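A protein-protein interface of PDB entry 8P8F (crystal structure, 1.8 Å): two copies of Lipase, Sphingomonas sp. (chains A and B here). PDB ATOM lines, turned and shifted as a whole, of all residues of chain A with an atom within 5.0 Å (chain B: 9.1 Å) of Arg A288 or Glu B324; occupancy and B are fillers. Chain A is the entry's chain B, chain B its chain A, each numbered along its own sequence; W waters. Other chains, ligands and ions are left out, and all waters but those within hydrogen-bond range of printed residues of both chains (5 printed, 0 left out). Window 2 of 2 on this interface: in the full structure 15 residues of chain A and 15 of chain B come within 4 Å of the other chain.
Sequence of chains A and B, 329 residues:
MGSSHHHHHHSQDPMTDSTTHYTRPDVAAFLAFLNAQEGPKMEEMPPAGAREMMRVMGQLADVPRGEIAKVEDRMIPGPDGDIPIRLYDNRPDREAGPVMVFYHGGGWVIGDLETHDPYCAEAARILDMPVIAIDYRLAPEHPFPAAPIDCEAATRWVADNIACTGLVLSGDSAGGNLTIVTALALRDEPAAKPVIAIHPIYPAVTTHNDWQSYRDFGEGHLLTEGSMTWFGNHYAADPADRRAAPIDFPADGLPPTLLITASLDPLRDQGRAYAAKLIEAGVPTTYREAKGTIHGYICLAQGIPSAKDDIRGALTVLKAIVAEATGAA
Of the printed residues of chain B, Thr A286 touches Thr B285 (3.7 Å) and Thr B286 (3.6 Å).
Of chain B, only Ile B279, Val B283, Pro B284 and Thr B285 come within 4 Å of Tyr A287.
Of chain B, only Glu B324 (3.1 Å) comes within 4 Å of Arg A288.
Gly A313 touches none of the printed residues of chain B.
Of the printed residues of chain A, Ile B279 touches Tyr A287.
Of the printed residues of chain A, Val B283 touches Tyr A287 (3.8 Å).
Printed residues of chain A within 4 Å of Thr B285: Thr A286 (3.7 Å) and Tyr A287 (2.8 Å).
Printed residues of chain A within 4 Å of Thr B286: Thr A286.
Of chain A, only Arg A288 (3.1 Å) comes within 4 Å of Glu B324.
Ala B325 touches none of the printed residues of chain A.
The nearest residue of chain A that does not touch Glu B324 is Gly A313 (4.6 Å).
The nearest printed residue of chain A that does not touch Ile B279 is Glu A289 (4.8 Å).
Thr A286 touches its own counterpart, Thr B286.
3 positions are printed for both chains.
The backbone carbonyl oxygen of Thr B257 lies within hydrogen-bond range of the backbone NH of Thr B286 (2.8 Å).
OG1 of Thr B285 is in hydrogen-bond range of O of Val B283 (2.7 Å).
The backbone carbonyl oxygen of Thr A286 lies within hydrogen-bond range of the backbone NH of Leu A259.
The backbone carbonyl oxygen (O) of Leu A259 lies within hydrogen-bond range of the backbone NH (N) of Arg A288 (3.0 Å).
OG1 of Thr A261 is in hydrogen-bond range of OH of Tyr A287, 2.6 Å away.
OH of Tyr A287 is in hydrogen-bond range of OE1 of Glu A289, 2.5 Å away.
The backbone NH (N) of Tyr A287 is in hydrogen-bond range of the backbone carbonyl oxygen (O) of Thr B285 (2.8 Å).
NH1 of Arg A288 is in salt-bridge range of OE1 of Glu B324 (3.1 Å).
Among the printed residues, pairs that only touch across the chains: Glu A289 with Gly B282 (3.5 Å), Thr A286 with Thr B286 (3.6 Å), Tyr A287 with Ile B279 (3.6 Å), Tyr A287 with Pro B284 (3.6 Å), Thr A286 with Thr B285 (3.7 Å) and Tyr A287 with Val B283 (3.8 Å).
Hydrophobic or aromatic side chains of chain B within 4 Å of the printed part of chain A: Ile B279.
Printed residues of chain A that touch a printed residue of chain B: Thr A286, Tyr A287, Arg A288 and Glu A289.
Hydrophobic or aromatic side chains of chain A within 4 Å of the printed part of chain B: Tyr A287.
Among the printed residues, Asp or Glu carboxylates within 4 Å of a Lys or Arg side-chain nitrogen of the other chain: Arg A288 with Glu B324.
Water W5 lies within hydrogen-bond range of the backbone carbonyl oxygen (O) of Tyr A287 and the backbone NH (N) of Thr B285.
Water W2 bridges the side-chain carboxylate of Glu B324 (2.6 Å) and the backbone carbonyl oxygen of Gly A313 (2.8 Å).
Water W4 bridges the side-chain carboxylate of Glu B324 (2.6 Å) and the guanidinium group of Arg A288 (3.4 Å).
Water W1 bridges O of Tyr B287 (2.8 Å) and OG1 of Thr A286 (3.5 Å).
Water W3 lies within hydrogen-bond range of the side-chain carboxylate (OE2) of Glu B324 (3.0 Å) and the guanidinium group (NH1) of Arg A288 (3.2 Å).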
ATOM      1  N   LEU A 258     -18.609 -20.222  -0.369  1.00  0.00           N
ATOM      2  CA  LEU A 258     -19.474 -20.460   0.773  1.00  0.00           C
ATOM      3  C   LEU A 258     -20.884 -19.981   0.408  1.00  0.00           C
ATOM      4  O   LEU A 258     -21.066 -18.775   0.125  1.00  0.00           O
ATOM      5  CB  LEU A 258     -18.962 -19.644   1.946  1.00  0.00           C
ATOM      6  CG  LEU A 258     -19.900 -19.648   3.166  1.00  0.00           C
ATOM      7  CD1 LEU A 258     -20.114 -21.103   3.680  1.00  0.00           C
ATOM      8  CD2 LEU A 258     -19.345 -18.758   4.272  1.00  0.00           C
ATOM      9  N   LEU A 259     -21.835 -20.895   0.211  1.00  0.00           N
ATOM     10  CA  LEU A 259     -23.187 -20.448  -0.187  1.00  0.00           C
ATOM     11  C   LEU A 259     -24.149 -20.808   0.925  1.00  0.00           C
ATOM     12  O   LEU A 259     -24.127 -21.933   1.431  1.00  0.00           O
ATOM     13  CB  LEU A 259     -23.539 -21.155  -1.495  1.00  0.00           C
ATOM     14  CG  LEU A 259     -24.830 -20.676  -2.187  1.00  0.00           C
ATOM     15  CD1 LEU A 259     -24.694 -21.006  -3.709  1.00  0.00           C
ATOM     16  CD2 LEU A 259     -26.031 -21.370  -1.656  1.00  0.00           C
ATOM     17  N   ILE A 260     -24.941 -19.828   1.370  1.00  0.00           N
ATOM     18  CA  ILE A 260     -25.882 -20.023   2.458  1.00  0.00           C
ATOM     19  C   ILE A 260     -27.281 -19.710   1.925  1.00  0.00           C
ATOM     20  O   ILE A 260     -27.439 -18.780   1.127  1.00  0.00           O
ATOM     21  CB  ILE A 260     -25.481 -19.276   3.746  1.00  0.00           C
ATOM     22  CG1 ILE A 260     -26.391 -19.682   4.920  1.00  0.00           C
ATOM     23  CG2 ILE A 260     -25.479 -17.763   3.536  1.00  0.00           C
ATOM     24  CD1 ILE A 260     -25.815 -19.337   6.276  1.00  0.00           C
ATOM     25  N   THR A 261     -28.221 -20.547   2.346  1.00  0.00           N
ATOM     26  CA  THR A 261     -29.630 -20.387   2.071  1.00  0.00           C
ATOM     27  C   THR A 261     -30.355 -20.219   3.406  1.00  0.00           C
ATOM     28  O   THR A 261     -29.797 -20.423   4.524  1.00  0.00           O
ATOM     29  CB  THR A 261     -30.239 -21.477   1.201  1.00  0.00           C
ATOM     30  OG1 THR A 261     -30.178 -22.670   2.013  1.00  0.00           O
ATOM     31  CG2 THR A 261     -29.576 -21.676  -0.148  1.00  0.00           C
ATOM     32  N   THR A 286     -18.726 -24.870   0.397  1.00  0.00           N
ATOM     33  CA  THR A 286     -19.344 -25.100   1.672  1.00  0.00           C
ATOM     34  C   THR A 286     -20.780 -24.609   1.594  1.00  0.00           C
ATOM     35  O   THR A 286     -20.987 -23.435   1.261  1.00  0.00           O
ATOM     36  CB  THR A 286     -18.559 -24.373   2.757  1.00  0.00           C
ATOM     37  OG1 THR A 286     -17.186 -24.769   2.662  1.00  0.00           O
ATOM     38  CG2 THR A 286     -19.139 -24.657   4.124  1.00  0.00           C
ATOM     39  N   TYR A 287     -21.713 -25.507   1.838  1.00  0.00           N
ATOM     40  CA  TYR A 287     -23.123 -25.207   1.779  1.00  0.00           C
ATOM     41  C   TYR A 287     -23.629 -25.131   3.210  1.00  0.00           C
ATOM     42  O   TYR A 287     -23.556 -26.133   3.970  1.00  0.00           O
ATOM     43  CB  TYR A 287     -23.843 -26.266   0.981  1.00  0.00           C
ATOM     44  CG  TYR A 287     -25.329 -25.981   0.988  1.00  0.00           C
ATOM     45  CD1 TYR A 287     -25.848 -24.891   0.324  1.00  0.00           C
ATOM     46  CD2 TYR A 287     -26.194 -26.740   1.738  1.00  0.00           C
ATOM     47  CE1 TYR A 287     -27.200 -24.588   0.391  1.00  0.00           C
ATOM     48  CE2 TYR A 287     -27.550 -26.454   1.803  1.00  0.00           C
ATOM     49  CZ  TYR A 287     -28.045 -25.377   1.114  1.00  0.00           C
ATOM     50  OH  TYR A 287     -29.363 -25.023   1.192  1.00  0.00           O
ATOM     51  N   ARG A 288     -24.279 -24.020   3.557  1.00  0.00           N
ATOM     52  CA  ARG A 288     -24.913 -23.886   4.844  1.00  0.00           C
ATOM     53  C   ARG A 288     -26.391 -23.550   4.581  1.00  0.00           C
ATOM     54  O   ARG A 288     -26.736 -22.882   3.586  1.00  0.00           O
ATOM     55  CB  ARG A 288     -24.268 -22.777   5.709  1.00  0.00           C
ATOM     56  CG  ARG A 288     -22.803 -23.046   6.030  1.00  0.00           C
ATOM     57  CD  ARG A 288     -22.126 -21.925   6.756  1.00  0.00           C
ATOM     58  NE  ARG A 288     -22.768 -21.578   8.044  1.00  0.00           N
ATOM     59  CZ  ARG A 288     -22.459 -22.141   9.217  1.00  0.00           C
ATOM     60  NH1 ARG A 288     -21.677 -23.187   9.246  1.00  0.00           N
ATOM     61  NH2 ARG A 288     -23.054 -21.737  10.343  1.00  0.00           N
ATOM     62  N   GLU A 289     -27.261 -24.070   5.431  1.00  0.00           N
ATOM     63  CA  GLU A 289     -28.682 -23.752   5.326  1.00  0.00           C
ATOM     64  C   GLU A 289     -29.133 -23.293   6.714  1.00  0.00           C
ATOM     65  O   GLU A 289     -29.111 -24.047   7.655  1.00  0.00           O
ATOM     66  CB  GLU A 289     -29.425 -24.944   4.739  1.00  0.00           C
ATOM     67  CG  GLU A 289     -30.906 -24.672   4.555  1.00  0.00           C
ATOM     68  CD  GLU A 289     -31.624 -25.690   3.670  1.00  0.00           C
ATOM     69  OE1 GLU A 289     -31.013 -26.199   2.622  1.00  0.00           O
ATOM     70  OE2 GLU A 289     -32.777 -26.076   4.084  1.00  0.00           O
ATOM     71  N   ALA A 290     -29.563 -22.072   6.821  1.00  0.00           N
ATOM     72  CA  ALA A 290     -30.054 -21.464   8.055  1.00  0.00           C
ATOM     73  C   ALA A 290     -31.454 -22.005   8.350  1.00  0.00           C
ATOM     74  O   ALA A 290     -32.410 -21.620   7.662  1.00  0.00           O
ATOM     75  CB  ALA A 290     -29.994 -19.964   7.838  1.00  0.00           C
ATOM     76  N   GLY A 313     -21.933 -17.375  12.397  1.00  0.00           N
ATOM     77  CA  GLY A 313     -21.599 -18.745  12.007  1.00  0.00           C
ATOM     78  C   GLY A 313     -21.015 -18.810  10.586  1.00  0.00           C
ATOM     79  O   GLY A 313     -19.990 -19.484  10.312  1.00  0.00           O
ATOM     80  N   ALA A 314     -21.679 -18.099   9.657  1.00  0.00           N
ATOM     81  CA  ALA A 314     -21.232 -18.059   8.256  1.00  0.00           C
ATOM     82  C   ALA A 314     -19.857 -17.354   8.152  1.00  0.00           C
ATOM     83  O   ALA A 314     -18.964 -17.779   7.429  1.00  0.00           O
ATOM     84  CB  ALA A 314     -22.264 -17.411   7.346  1.00  0.00           C
ATOM     85  N   VAL A 317     -16.842 -19.347   9.219  1.00  0.00           N
ATOM     86  CA  VAL A 317     -16.515 -20.319   8.208  1.00  0.00           C
ATOM     87  C   VAL A 317     -15.772 -19.646   7.064  1.00  0.00           C
ATOM     88  O   VAL A 317     -14.733 -20.155   6.549  1.00  0.00           O
ATOM     89  CB  VAL A 317     -17.745 -21.106   7.754  1.00  0.00           C
ATOM     90  CG1 VAL A 317     -17.433 -21.896   6.459  1.00  0.00           C
ATOM     91  CG2 VAL A 317     -18.177 -22.042   8.867  1.00  0.00           C
ATOM     92  N   PRO B  98     -17.838 -35.589  21.998  1.00  0.00           N
ATOM     93  CA  PRO B  98     -18.050 -36.411  20.815  1.00  0.00           C
ATOM     94  C   PRO B  98     -16.909 -37.399  20.702  1.00  0.00           C
ATOM     95  O   PRO B  98     -15.842 -37.234  21.310  1.00  0.00           O
ATOM     96  CB  PRO B  98     -18.149 -35.384  19.702  1.00  0.00           C
ATOM     97  CG  PRO B  98     -17.660 -34.092  20.228  1.00  0.00           C
ATOM     98  CD  PRO B  98     -17.655 -34.169  21.715  1.00  0.00           C
ATOM     99  N   ILE B 196     -23.551 -36.522  15.142  1.00  0.00           N
ATOM    100  CA  ILE B 196     -23.467 -35.090  14.988  1.00  0.00           C
ATOM    101  C   ILE B 196     -22.836 -34.631  13.698  1.00  0.00           C
ATOM    102  O   ILE B 196     -23.064 -33.480  13.337  1.00  0.00           O
ATOM    103  CB  ILE B 196     -22.913 -34.396  16.245  1.00  0.00           C
ATOM    104  CG1 ILE B 196     -21.417 -34.608  16.386  1.00  0.00           C
ATOM    105  CG2 ILE B 196     -23.708 -34.828  17.486  1.00  0.00           C
ATOM    106  CD1 ILE B 196     -20.913 -34.075  17.713  1.00  0.00           C
ATOM    107  N   ALA B 197     -22.030 -35.498  13.040  1.00  0.00           N
ATOM    108  CA  ALA B 197     -21.400 -35.136  11.782  1.00  0.00           C
ATOM    109  C   ALA B 197     -20.789 -36.388  11.198  1.00  0.00           C
ATOM    110  O   ALA B 197     -20.596 -37.374  11.927  1.00  0.00           O
ATOM    111  CB  ALA B 197     -20.319 -34.100  11.977  1.00  0.00           C
ATOM    112  N   PRO B 256     -24.637 -33.177   9.350  1.00  0.00           N
ATOM    113  CA  PRO B 256     -23.715 -32.274   8.660  1.00  0.00           C
ATOM    114  C   PRO B 256     -22.557 -33.144   8.151  1.00  0.00           C
ATOM    115  O   PRO B 256     -22.098 -34.020   8.892  1.00  0.00           O
ATOM    116  CB  PRO B 256     -23.242 -31.319   9.732  1.00  0.00           C
ATOM    117  CG  PRO B 256     -24.432 -31.266  10.702  1.00  0.00           C
ATOM    118  CD  PRO B 256     -24.994 -32.664  10.695  1.00  0.00           C
ATOM    119  N   THR B 257     -22.238 -32.980   6.884  1.00  0.00           N
ATOM    120  CA  THR B 257     -21.273 -33.849   6.187  1.00  0.00           C
ATOM    121  C   THR B 257     -20.063 -33.033   5.722  1.00  0.00           C
ATOM    122  O   THR B 257     -20.174 -31.945   5.108  1.00  0.00           O
ATOM    123  CB  THR B 257     -21.990 -34.500   4.985  1.00  0.00           C
ATOM    124  OG1 THR B 257     -23.062 -35.311   5.490  1.00  0.00           O
ATOM    125  CG2 THR B 257     -21.036 -35.312   4.113  1.00  0.00           C
ATOM    126  N   ILE B 279     -26.801 -31.775  -0.654  1.00  0.00           N
ATOM    127  CA  ILE B 279     -27.223 -30.366  -0.703  1.00  0.00           C
ATOM    128  C   ILE B 279     -28.638 -30.214  -1.179  1.00  0.00           C
ATOM    129  O   ILE B 279     -29.445 -29.489  -0.537  1.00  0.00           O
ATOM    130  CB  ILE B 279     -26.213 -29.614  -1.557  1.00  0.00           C
ATOM    131  CG1 ILE B 279     -24.870 -29.582  -0.778  1.00  0.00           C
ATOM    132  CG2 ILE B 279     -26.721 -28.244  -1.939  1.00  0.00           C
ATOM    133  CD1 ILE B 279     -23.748 -28.875  -1.502  1.00  0.00           C
ATOM    134  N   GLY B 282     -31.025 -30.652   1.441  1.00  0.00           N
ATOM    135  CA  GLY B 282     -31.029 -29.720   2.560  1.00  0.00           C
ATOM    136  C   GLY B 282     -30.029 -30.110   3.655  1.00  0.00           C
ATOM    137  O   GLY B 282     -30.106 -29.589   4.773  1.00  0.00           O
ATOM    138  N   VAL B 283     -29.100 -31.019   3.369  1.00  0.00           N
ATOM    139  CA  VAL B 283     -28.086 -31.374   4.341  1.00  0.00           C
ATOM    140  C   VAL B 283     -26.903 -30.408   4.285  1.00  0.00           C
ATOM    141  O   VAL B 283     -26.320 -30.259   3.220  1.00  0.00           O
ATOM    142  CB  VAL B 283     -27.589 -32.815   4.167  1.00  0.00           C
ATOM    143  CG1 VAL B 283     -26.548 -33.198   5.182  1.00  0.00           C
ATOM    144  CG2 VAL B 283     -28.726 -33.806   4.220  1.00  0.00           C
ATOM    145  N   PRO B 284     -26.481 -29.788   5.429  1.00  0.00           N
ATOM    146  CA  PRO B 284     -25.319 -28.899   5.472  1.00  0.00           C
ATOM    147  C   PRO B 284     -24.077 -29.724   5.115  1.00  0.00           C
ATOM    148  O   PRO B 284     -23.884 -30.809   5.684  1.00  0.00           O
ATOM    149  CB  PRO B 284     -25.168 -28.385   6.891  1.00  0.00           C
ATOM    150  CG  PRO B 284     -26.457 -28.811   7.610  1.00  0.00           C
ATOM    151  CD  PRO B 284     -27.143 -29.843   6.745  1.00  0.00           C
ATOM    152  N   THR B 285     -23.366 -29.274   4.134  1.00  0.00           N
ATOM    153  CA  THR B 285     -22.366 -30.108   3.406  1.00  0.00           C
ATOM    154  C   THR B 285     -21.179 -29.236   3.071  1.00  0.00           C
ATOM    155  O   THR B 285     -21.320 -28.184   2.416  1.00  0.00           O
ATOM    156  CB  THR B 285     -22.912 -30.726   2.107  1.00  0.00           C
ATOM    157  OG1 THR B 285     -24.049 -31.518   2.369  1.00  0.00           O
ATOM    158  CG2 THR B 285     -21.941 -31.591   1.333  1.00  0.00           C
ATOM    159  N   THR B 286     -19.978 -29.691   3.446  1.00  0.00           N
ATOM    160  CA  THR B 286     -18.753 -29.099   3.027  1.00  0.00           C
ATOM    161  C   THR B 286     -18.025 -30.068   2.089  1.00  0.00           C
ATOM    162  O   THR B 286     -17.784 -31.205   2.483  1.00  0.00           O
ATOM    163  CB  THR B 286     -17.879 -28.837   4.256  1.00  0.00           C
ATOM    164  OG1 THR B 286     -18.586 -28.007   5.200  1.00  0.00           O
ATOM    165  CG2 THR B 286     -16.578 -28.170   3.956  1.00  0.00           C
ATOM    166  N   TYR B 287     -17.786 -29.575   0.875  1.00  0.00           N
ATOM    167  CA  TYR B 287     -17.142 -30.387  -0.158  1.00  0.00           C
ATOM    168  C   TYR B 287     -15.736 -29.895  -0.315  1.00  0.00           C
ATOM    169  O   TYR B 287     -15.554 -28.712  -0.599  1.00  0.00           O
ATOM    170  CB  TYR B 287     -17.973 -30.338  -1.417  1.00  0.00           C
ATOM    171  CG  TYR B 287     -17.246 -31.049  -2.532  1.00  0.00           C
ATOM    172  CD1 TYR B 287     -17.173 -32.406  -2.491  1.00  0.00           C
ATOM    173  CD2 TYR B 287     -16.543 -30.388  -3.502  1.00  0.00           C
ATOM    174  CE1 TYR B 287     -16.490 -33.142  -3.451  1.00  0.00           C
ATOM    175  CE2 TYR B 287     -15.856 -31.105  -4.477  1.00  0.00           C
ATOM    176  CZ  TYR B 287     -15.845 -32.486  -4.436  1.00  0.00           C
ATOM    177  OH  TYR B 287     -15.129 -33.271  -5.352  1.00  0.00           O
ATOM    178  N   VAL B 317     -11.202 -28.527   9.362  1.00  0.00           N
ATOM    179  CA  VAL B 317     -12.559 -28.186   8.957  1.00  0.00           C
ATOM    180  C   VAL B 317     -13.528 -29.038   9.750  1.00  0.00           C
ATOM    181  O   VAL B 317     -14.566 -28.512  10.223  1.00  0.00           O
ATOM    182  CB  VAL B 317     -12.720 -28.352   7.430  1.00  0.00           C
ATOM    183  CG1 VAL B 317     -14.151 -28.380   6.949  1.00  0.00           C
ATOM    184  CG2 VAL B 317     -11.927 -27.242   6.690  1.00  0.00           C
ATOM    185  N   LEU B 318     -13.252 -30.346   9.865  1.00  0.00           N
ATOM    186  CA  LEU B 318     -14.155 -31.205  10.653  1.00  0.00           C
ATOM    187  C   LEU B 318     -14.241 -30.784  12.148  1.00  0.00           C
ATOM    188  O   LEU B 318     -15.345 -30.768  12.763  1.00  0.00           O
ATOM    189  CB  LEU B 318     -13.783 -32.671  10.470  1.00  0.00           C
ATOM    190  CG  LEU B 318     -14.655 -33.673  11.251  1.00  0.00           C
ATOM    191  CD1 LEU B 318     -16.053 -33.693  10.795  1.00  0.00           C
ATOM    192  CD2 LEU B 318     -14.101 -35.037  11.108  1.00  0.00           C
ATOM    193  N   LYS B 319     -13.085 -30.428  12.722  1.00  0.00           N
ATOM    194  CA  LYS B 319     -13.044 -29.965  14.114  1.00  0.00           C
ATOM    195  C   LYS B 319     -13.985 -28.785  14.364  1.00  0.00           C
ATOM    196  O   LYS B 319     -14.786 -28.734  15.325  1.00  0.00           O
ATOM    197  CB  LYS B 319     -11.615 -29.679  14.494  1.00  0.00           C
ATOM    198  CG  LYS B 319     -11.382 -29.379  15.997  1.00  0.00           C
ATOM    199  CD  LYS B 319      -9.952 -29.080  16.407  1.00  0.00           C
ATOM    200  CE  LYS B 319      -9.865 -29.136  17.918  1.00  0.00           C
ATOM    201  NZ  LYS B 319      -8.475 -29.027  18.360  1.00  0.00           N
ATOM    202  N   ALA B 320     -13.999 -27.842  13.413  1.00  0.00           N
ATOM    203  CA  ALA B 320     -14.897 -26.704  13.411  1.00  0.00           C
ATOM    204  C   ALA B 320     -16.357 -27.111  13.225  1.00  0.00           C
ATOM    205  O   ALA B 320     -17.251 -26.539  13.895  1.00  0.00           O
ATOM    206  CB  ALA B 320     -14.474 -25.716  12.329  1.00  0.00           C
ATOM    207  N   ILE B 321     -16.626 -28.122  12.383  1.00  0.00           N
ATOM    208  CA  ILE B 321     -18.006 -28.546  12.198  1.00  0.00           C
ATOM    209  C   ILE B 321     -18.546 -29.092  13.526  1.00  0.00           C
ATOM    210  O   ILE B 321     -19.664 -28.782  13.951  1.00  0.00           O
ATOM    211  CB  ILE B 321     -18.074 -29.590  11.068  1.00  0.00           C
ATOM    212  CG1 ILE B 321     -17.975 -28.912   9.710  1.00  0.00           C
ATOM    213  CG2 ILE B 321     -19.349 -30.387  11.127  1.00  0.00           C
ATOM    214  CD1 ILE B 321     -17.830 -29.904   8.541  1.00  0.00           C
ATOM    215  N   VAL B 322     -17.666 -29.865  14.194  1.00  0.00           N
ATOM    216  CA  VAL B 322     -18.037 -30.483  15.448  1.00  0.00           C
ATOM    217  C   VAL B 322     -18.165 -29.410  16.551  1.00  0.00           C
ATOM    218  O   VAL B 322     -19.141 -29.458  17.315  1.00  0.00           O
ATOM    219  CB  VAL B 322     -17.058 -31.604  15.796  1.00  0.00           C
ATOM    220  CG1 VAL B 322     -17.329 -32.144  17.154  1.00  0.00           C
ATOM    221  CG2 VAL B 322     -17.083 -32.724  14.785  1.00  0.00           C
ATOM    222  N   ALA B 323     -17.289 -28.390  16.606  1.00  0.00           N
ATOM    223  CA  ALA B 323     -17.357 -27.331  17.612  1.00  0.00           C
ATOM    224  C   ALA B 323     -18.625 -26.523  17.457  1.00  0.00           C
ATOM    225  O   ALA B 323     -19.225 -26.101  18.451  1.00  0.00           O
ATOM    226  CB  ALA B 323     -16.186 -26.397  17.595  1.00  0.00           C
ATOM    227  N   GLU B 324     -19.081 -26.335  16.204  1.00  0.00           N
ATOM    228  CA  GLU B 324     -20.343 -25.642  15.982  1.00  0.00           C
ATOM    229  C   GLU B 324     -21.514 -26.474  16.494  1.00  0.00           C
ATOM    230  O   GLU B 324     -22.459 -25.925  17.073  1.00  0.00           O
ATOM    231  CB  GLU B 324     -20.481 -25.329  14.491  1.00  0.00           C
ATOM    232  CG  GLU B 324     -21.791 -24.696  14.123  1.00  0.00           C
ATOM    233  CD  GLU B 324     -21.821 -24.402  12.639  1.00  0.00           C
ATOM    234  OE1 GLU B 324     -21.072 -23.540  12.221  1.00  0.00           O
ATOM    235  OE2 GLU B 324     -22.546 -25.103  11.935  1.00  0.00           O
ATOM    236  N   ALA B 325     -21.490 -27.778  16.214  1.00  0.00           N
ATOM    237  CA  ALA B 325     -22.542 -28.668  16.664  1.00  0.00           C
ATOM    238  C   ALA B 325     -22.622 -28.666  18.188  1.00  0.00           C
ATOM    239  O   ALA B 325     -23.691 -28.476  18.742  1.00  0.00           O
ATOM    240  CB  ALA B 325     -22.319 -30.055  16.162  1.00  0.00           C
ATOM    241  N   THR B 326     -21.449 -28.751  18.821  1.00  0.00           N
ATOM    242  CA  THR B 326     -21.323 -28.802  20.301  1.00  0.00           C
ATOM    243  C   THR B 326     -21.709 -27.474  20.973  1.00  0.00           C
ATOM    244  O   THR B 326     -22.244 -27.534  22.078  1.00  0.00           O
ATOM    245  CB  THR B 326     -19.892 -29.249  20.645  1.00  0.00           C
ATOM    246  OG1 THR B 326     -18.971 -28.274  20.165  1.00  0.00           O
ATOM    247  CG2 THR B 326     -19.557 -30.606  20.068  1.00  0.00           C
ATOM    248  N   GLY B 327     -21.460 -26.337  20.328  1.00  0.00           N
ATOM    249  CA  GLY B 327     -21.796 -25.021  20.900  1.00  0.00           C
ATOM    250  C   GLY B 327     -23.229 -24.599  20.616  1.00  0.00           C
ATOM    251  O   GLY B 327     -23.616 -23.511  21.052  1.00  0.00           O
ATOM    252  N   ALA B 328     -23.983 -25.427  19.902  1.00  0.00           N
ATOM    253  CA  ALA B 328     -25.440 -25.260  19.729  1.00  0.00           C
ATOM    254  C   ALA B 328     -26.171 -26.103  20.773  1.00  0.00           C
ATOM    255  O   ALA B 328     -26.004 -27.329  20.723  1.00  0.00           O
ATOM    256  CB  ALA B 328     -25.830 -25.689  18.346  1.00  0.00           C
HETATM  257  O   HOH W   1     -14.772 -26.556   0.963  1.00  0.00           O
HETATM  258  O   HOH W   2     -19.566 -21.420  12.258  1.00  0.00           O
HETATM  259  O   HOH W   3     -20.288 -25.971  10.085  1.00  0.00           O
HETATM  260  O   HOH W   4     -24.913 -24.017  12.097  1.00  0.00           O
HETATM  261  O   HOH W   5     -21.881 -26.691   5.807  1.00  0.00           O
